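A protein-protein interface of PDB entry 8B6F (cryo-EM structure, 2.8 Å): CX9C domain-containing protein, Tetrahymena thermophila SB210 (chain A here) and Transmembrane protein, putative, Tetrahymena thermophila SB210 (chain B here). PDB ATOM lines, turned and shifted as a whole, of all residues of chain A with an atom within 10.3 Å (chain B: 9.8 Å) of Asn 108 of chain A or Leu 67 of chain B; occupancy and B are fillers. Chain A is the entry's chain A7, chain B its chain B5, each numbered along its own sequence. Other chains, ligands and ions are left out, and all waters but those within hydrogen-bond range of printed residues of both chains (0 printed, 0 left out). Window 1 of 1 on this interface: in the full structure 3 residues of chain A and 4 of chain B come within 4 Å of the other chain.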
ATOM      1  N   LYS A 106     -12.322   8.038   4.574  1.00  0.00           N
ATOM      2  CA  LYS A 106     -11.451   6.832   4.574  1.00  0.00           C
ATOM      3  C   LYS A 106     -11.575   6.114   3.242  1.00  0.00           C
ATOM      4  O   LYS A 106     -10.604   5.554   2.736  1.00  0.00           O
ATOM      5  CB  LYS A 106     -11.827   5.894   5.721  1.00  0.00           C
ATOM      6  CG  LYS A 106     -10.886   4.718   5.894  1.00  0.00           C
ATOM      7  CD  LYS A 106      -9.515   5.178   6.378  1.00  0.00           C
ATOM      8  CE  LYS A 106      -8.524   4.023   6.449  1.00  0.00           C
ATOM      9  NZ  LYS A 106      -7.906   3.727   5.131  1.00  0.00           N
ATOM     10  N   MET A 107     -12.783   6.132   2.678  1.00  0.00           N
ATOM     11  CA  MET A 107     -13.042   5.508   1.392  1.00  0.00           C
ATOM     12  C   MET A 107     -13.284   6.503   0.271  1.00  0.00           C
ATOM     13  O   MET A 107     -13.153   6.130  -0.899  1.00  0.00           O
ATOM     14  CB  MET A 107     -14.268   4.588   1.477  1.00  0.00           C
ATOM     15  CG  MET A 107     -14.137   3.452   2.464  1.00  0.00           C
ATOM     16  SD  MET A 107     -12.719   2.390   2.149  1.00  0.00           S
ATOM     17  CE  MET A 107     -12.965   1.970   0.427  1.00  0.00           C
ATOM     18  N   ASN A 108     -13.628   7.749   0.590  1.00  0.00           N
ATOM     19  CA  ASN A 108     -14.047   8.714  -0.418  1.00  0.00           C
ATOM     20  C   ASN A 108     -15.283   8.216  -1.165  1.00  0.00           C
ATOM     21  O   ASN A 108     -15.523   8.589  -2.314  1.00  0.00           O
ATOM     22  CB  ASN A 108     -12.907   9.021  -1.392  1.00  0.00           C
ATOM     23  CG  ASN A 108     -13.200  10.217  -2.273  1.00  0.00           C
ATOM     24  OD1 ASN A 108     -13.617  10.071  -3.420  1.00  0.00           O
ATOM     25  ND2 ASN A 108     -12.976  11.412  -1.738  1.00  0.00           N
ATOM     26  N   THR A 109     -16.073   7.368  -0.509  1.00  0.00           N
ATOM     27  CA  THR A 109     -17.280   6.794  -1.079  1.00  0.00           C
ATOM     28  C   THR A 109     -18.474   7.160  -0.209  1.00  0.00           C
ATOM     29  O   THR A 109     -18.363   7.259   1.015  1.00  0.00           O
ATOM     30  CB  THR A 109     -17.173   5.263  -1.191  1.00  0.00           C
ATOM     31  OG1 THR A 109     -15.975   4.913  -1.895  1.00  0.00           O
ATOM     32  CG2 THR A 109     -18.374   4.689  -1.928  1.00  0.00           C
ATOM     33  N   LYS A 110     -19.617   7.368  -0.853  1.00  0.00           N
ATOM     34  CA  LYS A 110     -20.814   7.769  -0.137  1.00  0.00           C
ATOM     35  C   LYS A 110     -21.468   6.562   0.536  1.00  0.00           C
ATOM     36  O   LYS A 110     -21.174   5.405   0.231  1.00  0.00           O
ATOM     37  CB  LYS A 110     -21.790   8.464  -1.080  1.00  0.00           C
ATOM     38  CG  LYS A 110     -21.190   9.661  -1.797  1.00  0.00           C
ATOM     39  CD  LYS A 110     -22.225  10.387  -2.636  1.00  0.00           C
ATOM     40  CE  LYS A 110     -21.669  11.688  -3.188  1.00  0.00           C
ATOM     41  NZ  LYS A 110     -22.686  12.438  -3.976  1.00  0.00           N
ATOM     42  N   SER A 111     -22.386   6.854   1.459  1.00  0.00           N
ATOM     43  CA  SER A 111     -22.883   5.828   2.371  1.00  0.00           C
ATOM     44  C   SER A 111     -23.624   4.722   1.631  1.00  0.00           C
ATOM     45  O   SER A 111     -23.344   3.534   1.827  1.00  0.00           O
ATOM     46  CB  SER A 111     -23.793   6.468   3.417  1.00  0.00           C
ATOM     47  OG  SER A 111     -24.257   5.498   4.339  1.00  0.00           O
ATOM     48  N   PHE A 112     -24.582   5.088   0.777  1.00  0.00           N
ATOM     49  CA  PHE A 112     -25.403   4.075   0.122  1.00  0.00           C
ATOM     50  C   PHE A 112     -24.568   3.209  -0.814  1.00  0.00           C
ATOM     51  O   PHE A 112     -24.776   1.993  -0.890  1.00  0.00           O
ATOM     52  CB  PHE A 112     -26.567   4.732  -0.624  1.00  0.00           C
ATOM     53  CG  PHE A 112     -27.547   5.447   0.279  1.00  0.00           C
ATOM     54  CD1 PHE A 112     -27.468   5.332   1.658  1.00  0.00           C
ATOM     55  CD2 PHE A 112     -28.562   6.221  -0.260  1.00  0.00           C
ATOM     56  CE1 PHE A 112     -28.370   5.985   2.475  1.00  0.00           C
ATOM     57  CE2 PHE A 112     -29.464   6.874   0.550  1.00  0.00           C
ATOM     58  CZ  PHE A 112     -29.370   6.757   1.918  1.00  0.00           C
ATOM     59  N   GLU A 113     -23.619   3.811  -1.530  1.00  0.00           N
ATOM     60  CA  GLU A 113     -22.709   3.021  -2.354  1.00  0.00           C
ATOM     61  C   GLU A 113     -21.875   2.079  -1.496  1.00  0.00           C
ATOM     62  O   GLU A 113     -21.589   0.947  -1.901  1.00  0.00           O
ATOM     63  CB  GLU A 113     -21.809   3.942  -3.174  1.00  0.00           C
ATOM     64  CG  GLU A 113     -22.569   4.837  -4.135  1.00  0.00           C
ATOM     65  CD  GLU A 113     -21.653   5.732  -4.935  1.00  0.00           C
ATOM     66  OE1 GLU A 113     -20.424   5.638  -4.746  1.00  0.00           O
ATOM     67  OE2 GLU A 113     -22.160   6.530  -5.750  1.00  0.00           O
ATOM     68  N   VAL A 114     -21.474   2.528  -0.307  1.00  0.00           N
ATOM     69  CA  VAL A 114     -20.735   1.658   0.604  1.00  0.00           C
ATOM     70  C   VAL A 114     -21.593   0.467   1.005  1.00  0.00           C
ATOM     71  O   VAL A 114     -21.112  -0.671   1.065  1.00  0.00           O
ATOM     72  CB  VAL A 114     -20.248   2.453   1.830  1.00  0.00           C
ATOM     73  CG1 VAL A 114     -19.790   1.518   2.944  1.00  0.00           C
ATOM     74  CG2 VAL A 114     -19.110   3.379   1.440  1.00  0.00           C
ATOM     75  N   HIS A 117     -21.797  -1.967  -1.982  1.00  0.00           N
ATOM     76  CA  HIS A 117     -20.552  -2.713  -2.127  1.00  0.00           C
ATOM     77  C   HIS A 117     -20.386  -3.732  -1.009  1.00  0.00           C
ATOM     78  O   HIS A 117     -19.930  -4.856  -1.246  1.00  0.00           O
ATOM     79  CB  HIS A 117     -19.364  -1.753  -2.156  1.00  0.00           C
ATOM     80  CG  HIS A 117     -19.136  -1.118  -3.491  1.00  0.00           C
ATOM     81  ND1 HIS A 117     -18.919   0.234  -3.646  1.00  0.00           N
ATOM     82  CD2 HIS A 117     -19.077  -1.652  -4.734  1.00  0.00           C
ATOM     83  CE1 HIS A 117     -18.745   0.506  -4.926  1.00  0.00           C
ATOM     84  NE2 HIS A 117     -18.835  -0.621  -5.608  1.00  0.00           N
ATOM     85  N   LEU A 157     -10.838  -2.975   6.067  1.00  0.00           N
ATOM     86  CA  LEU A 157     -10.927  -1.881   5.105  1.00  0.00           C
ATOM     87  C   LEU A 157     -10.045  -2.122   3.889  1.00  0.00           C
ATOM     88  O   LEU A 157     -10.431  -1.786   2.765  1.00  0.00           O
ATOM     89  CB  LEU A 157     -10.561  -0.558   5.774  1.00  0.00           C
ATOM     90  CG  LEU A 157     -11.531  -0.037   6.837  1.00  0.00           C
ATOM     91  CD1 LEU A 157     -11.031   1.288   7.373  1.00  0.00           C
ATOM     92  CD2 LEU A 157     -12.948   0.106   6.300  1.00  0.00           C
ATOM     93  N   TYR A 160     -11.867  -4.502   1.790  1.00  0.00           N
ATOM     94  CA  TYR A 160     -12.990  -3.807   1.174  1.00  0.00           C
ATOM     95  C   TYR A 160     -12.521  -2.969  -0.008  1.00  0.00           C
ATOM     96  O   TYR A 160     -13.195  -2.916  -1.043  1.00  0.00           O
ATOM     97  CB  TYR A 160     -13.698  -2.942   2.214  1.00  0.00           C
ATOM     98  CG  TYR A 160     -14.870  -2.174   1.664  1.00  0.00           C
ATOM     99  CD1 TYR A 160     -16.099  -2.788   1.466  1.00  0.00           C
ATOM    100  CD2 TYR A 160     -14.750  -0.831   1.346  1.00  0.00           C
ATOM    101  CE1 TYR A 160     -17.172  -2.085   0.964  1.00  0.00           C
ATOM    102  CE2 TYR A 160     -15.817  -0.122   0.845  1.00  0.00           C
ATOM    103  CZ  TYR A 160     -17.023  -0.753   0.655  1.00  0.00           C
ATOM    104  OH  TYR A 160     -18.083  -0.040   0.154  1.00  0.00           O
ATOM    105  N   LYS A 161     -11.371  -2.303   0.124  1.00  0.00           N
ATOM    106  CA  LYS A 161     -10.795  -1.605  -1.020  1.00  0.00           C
ATOM    107  C   LYS A 161     -10.557  -2.567  -2.174  1.00  0.00           C
ATOM    108  O   LYS A 161     -10.872  -2.258  -3.328  1.00  0.00           O
ATOM    109  CB  LYS A 161      -9.480  -0.933  -0.621  1.00  0.00           C
ATOM    110  CG  LYS A 161      -9.608   0.510  -0.184  1.00  0.00           C
ATOM    111  CD  LYS A 161      -9.803   0.633   1.316  1.00  0.00           C
ATOM    112  CE  LYS A 161      -9.559   2.058   1.780  1.00  0.00           C
ATOM    113  NZ  LYS A 161      -9.974   2.241   3.195  1.00  0.00           N
ATOM    114  N   GLU A 164     -14.028  -3.559  -3.742  1.00  0.00           N
ATOM    115  CA  GLU A 164     -14.869  -2.542  -4.366  1.00  0.00           C
ATOM    116  C   GLU A 164     -14.749  -2.531  -5.884  1.00  0.00           C
ATOM    117  O   GLU A 164     -15.663  -2.046  -6.560  1.00  0.00           O
ATOM    118  CB  GLU A 164     -14.525  -1.157  -3.817  1.00  0.00           C
ATOM    119  CG  GLU A 164     -15.357  -0.752  -2.612  1.00  0.00           C
ATOM    120  CD  GLU A 164     -15.257   0.730  -2.306  1.00  0.00           C
ATOM    121  OE1 GLU A 164     -14.242   1.349  -2.685  1.00  0.00           O
ATOM    122  OE2 GLU A 164     -16.197   1.277  -1.694  1.00  0.00           O
ATOM    123  N   ARG B  50     -14.853  23.636   3.408  1.00  0.00           N
ATOM    124  CA  ARG B  50     -15.842  23.944   2.378  1.00  0.00           C
ATOM    125  C   ARG B  50     -16.360  22.686   1.688  1.00  0.00           C
ATOM    126  O   ARG B  50     -16.720  22.715   0.510  1.00  0.00           O
ATOM    127  CB  ARG B  50     -15.272  24.922   1.346  1.00  0.00           C
ATOM    128  CG  ARG B  50     -14.979  26.299   1.924  1.00  0.00           C
ATOM    129  CD  ARG B  50     -14.374  27.234   0.891  1.00  0.00           C
ATOM    130  NE  ARG B  50     -15.270  27.479  -0.231  1.00  0.00           N
ATOM    131  CZ  ARG B  50     -15.054  28.381  -1.179  1.00  0.00           C
ATOM    132  NH1 ARG B  50     -13.984  29.157  -1.163  1.00  0.00           N
ATOM    133  NH2 ARG B  50     -15.935  28.509  -2.167  1.00  0.00           N
ATOM    134  N   TYR B  51     -16.404  21.570   2.415  1.00  0.00           N
ATOM    135  CA  TYR B  51     -17.056  20.369   1.914  1.00  0.00           C
ATOM    136  C   TYR B  51     -18.565  20.400   2.103  1.00  0.00           C
ATOM    137  O   TYR B  51     -19.262  19.553   1.534  1.00  0.00           O
ATOM    138  CB  TYR B  51     -16.487  19.129   2.607  1.00  0.00           C
ATOM    139  CG  TYR B  51     -15.061  18.815   2.228  1.00  0.00           C
ATOM    140  CD1 TYR B  51     -14.723  18.505   0.918  1.00  0.00           C
ATOM    141  CD2 TYR B  51     -14.056  18.809   3.184  1.00  0.00           C
ATOM    142  CE1 TYR B  51     -13.421  18.211   0.568  1.00  0.00           C
ATOM    143  CE2 TYR B  51     -12.750  18.515   2.844  1.00  0.00           C
ATOM    144  CZ  TYR B  51     -12.440  18.217   1.535  1.00  0.00           C
ATOM    145  OH  TYR B  51     -11.140  17.924   1.194  1.00  0.00           O
ATOM    146  N   SER B  52     -19.082  21.350   2.876  1.00  0.00           N
ATOM    147  CA  SER B  52     -20.508  21.502   3.115  1.00  0.00           C
ATOM    148  C   SER B  52     -20.982  22.822   2.525  1.00  0.00           C
ATOM    149  O   SER B  52     -20.327  23.856   2.683  1.00  0.00           O
ATOM    150  CB  SER B  52     -20.822  21.456   4.612  1.00  0.00           C
ATOM    151  OG  SER B  52     -22.216  21.587   4.840  1.00  0.00           O
ATOM    152  N   ILE B  63     -22.981  18.533  -8.776  1.00  0.00           N
ATOM    153  CA  ILE B  63     -23.338  17.225  -8.239  1.00  0.00           C
ATOM    154  C   ILE B  63     -22.053  16.455  -7.967  1.00  0.00           C
ATOM    155  O   ILE B  63     -21.262  16.200  -8.882  1.00  0.00           O
ATOM    156  CB  ILE B  63     -24.248  16.458  -9.210  1.00  0.00           C
ATOM    157  CG1 ILE B  63     -25.460  17.310  -9.602  1.00  0.00           C
ATOM    158  CG2 ILE B  63     -24.704  15.145  -8.590  1.00  0.00           C
ATOM    159  CD1 ILE B  63     -26.291  17.800  -8.431  1.00  0.00           C
ATOM    160  N   THR B  64     -21.842  16.083  -6.709  1.00  0.00           N
ATOM    161  CA  THR B  64     -20.610  15.429  -6.291  1.00  0.00           C
ATOM    162  C   THR B  64     -20.742  13.918  -6.430  1.00  0.00           C
ATOM    163  O   THR B  64     -21.686  13.320  -5.907  1.00  0.00           O
ATOM    164  CB  THR B  64     -20.269  15.795  -4.846  1.00  0.00           C
ATOM    165  OG1 THR B  64     -21.337  15.393  -3.979  1.00  0.00           O
ATOM    166  CG2 THR B  64     -20.048  17.293  -4.713  1.00  0.00           C
ATOM    167  N   LYS B  65     -19.791  13.310  -7.135  1.00  0.00           N
ATOM    168  CA  LYS B  65     -19.732  11.865  -7.296  1.00  0.00           C
ATOM    169  C   LYS B  65     -18.862  11.191  -6.244  1.00  0.00           C
ATOM    170  O   LYS B  65     -18.715   9.964  -6.277  1.00  0.00           O
ATOM    171  CB  LYS B  65     -19.207  11.512  -8.691  1.00  0.00           C
ATOM    172  CG  LYS B  65     -20.128  11.937  -9.822  1.00  0.00           C
ATOM    173  CD  LYS B  65     -19.504  11.640 -11.177  1.00  0.00           C
ATOM    174  CE  LYS B  65     -20.462  11.954 -12.314  1.00  0.00           C
ATOM    175  NZ  LYS B  65     -21.662  11.070 -12.299  1.00  0.00           N
ATOM    176  N   ASN B  66     -18.293  11.953  -5.315  1.00  0.00           N
ATOM    177  CA  ASN B  66     -17.418  11.422  -4.285  1.00  0.00           C
ATOM    178  C   ASN B  66     -17.836  11.977  -2.932  1.00  0.00           C
ATOM    179  O   ASN B  66     -18.555  12.974  -2.841  1.00  0.00           O
ATOM    180  CB  ASN B  66     -15.950  11.772  -4.556  1.00  0.00           C
ATOM    181  CG  ASN B  66     -15.376  11.004  -5.726  1.00  0.00           C
ATOM    182  OD1 ASN B  66     -15.802   9.888  -6.020  1.00  0.00           O
ATOM    183  ND2 ASN B  66     -14.402  11.599  -6.403  1.00  0.00           N
ATOM    184  N   LEU B  67     -17.374  11.310  -1.874  1.00  0.00           N
ATOM    185  CA  LEU B  67     -17.732  11.736  -0.527  1.00  0.00           C
ATOM    186  C   LEU B  67     -17.213  13.137  -0.233  1.00  0.00           C
ATOM    187  O   LEU B  67     -17.931  13.964   0.342  1.00  0.00           O
ATOM    188  CB  LEU B  67     -17.192  10.738   0.494  1.00  0.00           C
ATOM    189  CG  LEU B  67     -17.373  11.112   1.965  1.00  0.00           C
ATOM    190  CD1 LEU B  67     -18.826  11.422   2.283  1.00  0.00           C
ATOM    191  CD2 LEU B  67     -16.864   9.993   2.848  1.00  0.00           C
ATOM    192  N   TYR B  68     -15.973  13.425  -0.621  1.00  0.00           N
ATOM    193  CA  TYR B  68     -15.340  14.714  -0.365  1.00  0.00           C
ATOM    194  C   TYR B  68     -15.040  15.387  -1.697  1.00  0.00           C
ATOM    195  O   TYR B  68     -14.146  14.951  -2.430  1.00  0.00           O
ATOM    196  CB  TYR B  68     -14.061  14.545   0.452  1.00  0.00           C
ATOM    197  CG  TYR B  68     -14.262  13.845   1.773  1.00  0.00           C
ATOM    198  CD1 TYR B  68     -14.956  14.456   2.807  1.00  0.00           C
ATOM    199  CD2 TYR B  68     -13.743  12.578   1.991  1.00  0.00           C
ATOM    200  CE1 TYR B  68     -15.136  13.820   4.019  1.00  0.00           C
ATOM    201  CE2 TYR B  68     -13.916  11.932   3.197  1.00  0.00           C
ATOM    202  CZ  TYR B  68     -14.613  12.558   4.208  1.00  0.00           C
ATOM    203  OH  TYR B  68     -14.788  11.917   5.410  1.00  0.00           O
ATOM    204  N   GLU B  69     -15.785  16.445  -2.007  1.00  0.00           N
ATOM    205  CA  GLU B  69     -15.500  17.294  -3.156  1.00  0.00           C
ATOM    206  C   GLU B  69     -15.681  18.739  -2.725  1.00  0.00           C
ATOM    207  O   GLU B  69     -16.745  19.107  -2.221  1.00  0.00           O
ATOM    208  CB  GLU B  69     -16.414  16.966  -4.340  1.00  0.00           C
ATOM    209  CG  GLU B  69     -16.222  15.565  -4.899  1.00  0.00           C
ATOM    210  CD  GLU B  69     -16.943  15.358  -6.217  1.00  0.00           C
ATOM    211  OE1 GLU B  69     -17.476  16.345  -6.766  1.00  0.00           O
ATOM    212  OE2 GLU B  69     -16.975  14.210  -6.706  1.00  0.00           O
ATOM    213  N   LYS B  70     -14.647  19.553  -2.920  1.00  0.00           N
ATOM    214  CA  LYS B  70     -14.708  20.945  -2.499  1.00  0.00           C
ATOM    215  C   LYS B  70     -15.741  21.700  -3.323  1.00  0.00           C
ATOM    216  O   LYS B  70     -15.745  21.624  -4.556  1.00  0.00           O
ATOM    217  CB  LYS B  70     -13.334  21.599  -2.638  1.00  0.00           C
ATOM    218  CG  LYS B  70     -13.279  23.031  -2.129  1.00  0.00           C
ATOM    219  CD  LYS B  70     -11.881  23.612  -2.265  1.00  0.00           C
ATOM    220  CE  LYS B  70     -11.833  25.049  -1.771  1.00  0.00           C
ATOM    221  NZ  LYS B  70     -10.463  25.626  -1.875  1.00  0.00           N
ATOM    222  N   LEU B  71     -16.615  22.435  -2.641  1.00  0.00           N
ATOM    223  CA  LEU B  71     -17.667  23.193  -3.306  1.00  0.00           C
ATOM    224  C   LEU B  71     -17.284  24.662  -3.421  1.00  0.00           C
ATOM    225  O   LEU B  71     -16.486  25.168  -2.633  1.00  0.00           O
ATOM    226  CB  LEU B  71     -18.989  23.052  -2.548  1.00  0.00           C
ATOM    227  CG  LEU B  71     -19.519  21.626  -2.376  1.00  0.00           C
ATOM    228  CD1 LEU B  71     -20.791  21.630  -1.546  1.00  0.00           C
ATOM    229  CD2 LEU B  71     -19.764  20.963  -3.721  1.00  0.00           C
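Asn 108 of chain A touches three residues of chain B. Of the printed residues of chain A, Leu 67 of chain B touches Asn 108 (3.3 Å) and Thr 109 (3.6 Å). Tyr 68 of chain B touches just one residue of chain A: Asn 108. Of the printed residues of chain A, Thr 64 of chain B touches Lys 110. Printed residues of chain B within 4 Å of Lys 110 of chain A: Thr 64 (2.3 Å) and Asn 66 (3.4 Å). Glu 69 of chain B touches none of the printed residues of chain A. The nearest residue of chain B that does not touch Asn 108 of chain A is Lys 65 of chain B (5.3 Å).
OE2 of Glu 69 of chain B is in hydrogen-bond range of N of Asn 66 of chain B (3.0 Å). O of Met 107 of chain A is in hydrogen-bond range of OG1 of Thr 109 of chain A.
Hydrophobic or aromatic side chains of chain B that line the printed part of chain A: Leu 67 and Tyr 68. Printed residues of chain A that touch a printed residue of chain B: Asn 108, Thr 109 and Lys 110. Among the printed residues, 6 pairs touch across the chains.
The side-chain hydroxyl (OG1) of Thr 64 of chain B lies within hydrogen-bond range of the side-chain amino group (NZ) of Lys 110 of chain A, at 3.2 Å. The backbone NH of Leu 67 of chain B is in hydrogen-bond range of the backbone carbonyl oxygen of Asn 108 of chain A (3.3 Å). The side-chain amide oxygen (OD1) of Asn 66 of chain B lies close to the side-chain amide oxygen (OD1) of Asn 108 of chain A, 3.4 Å away.
Among the printed residues, merely in contact across the chains: Lys 110 of chain A with Asn 66 of chain B, Thr 109 of chain A with Leu 67 of chain B and Asn 108 of chain A with Tyr 68 of chain B.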
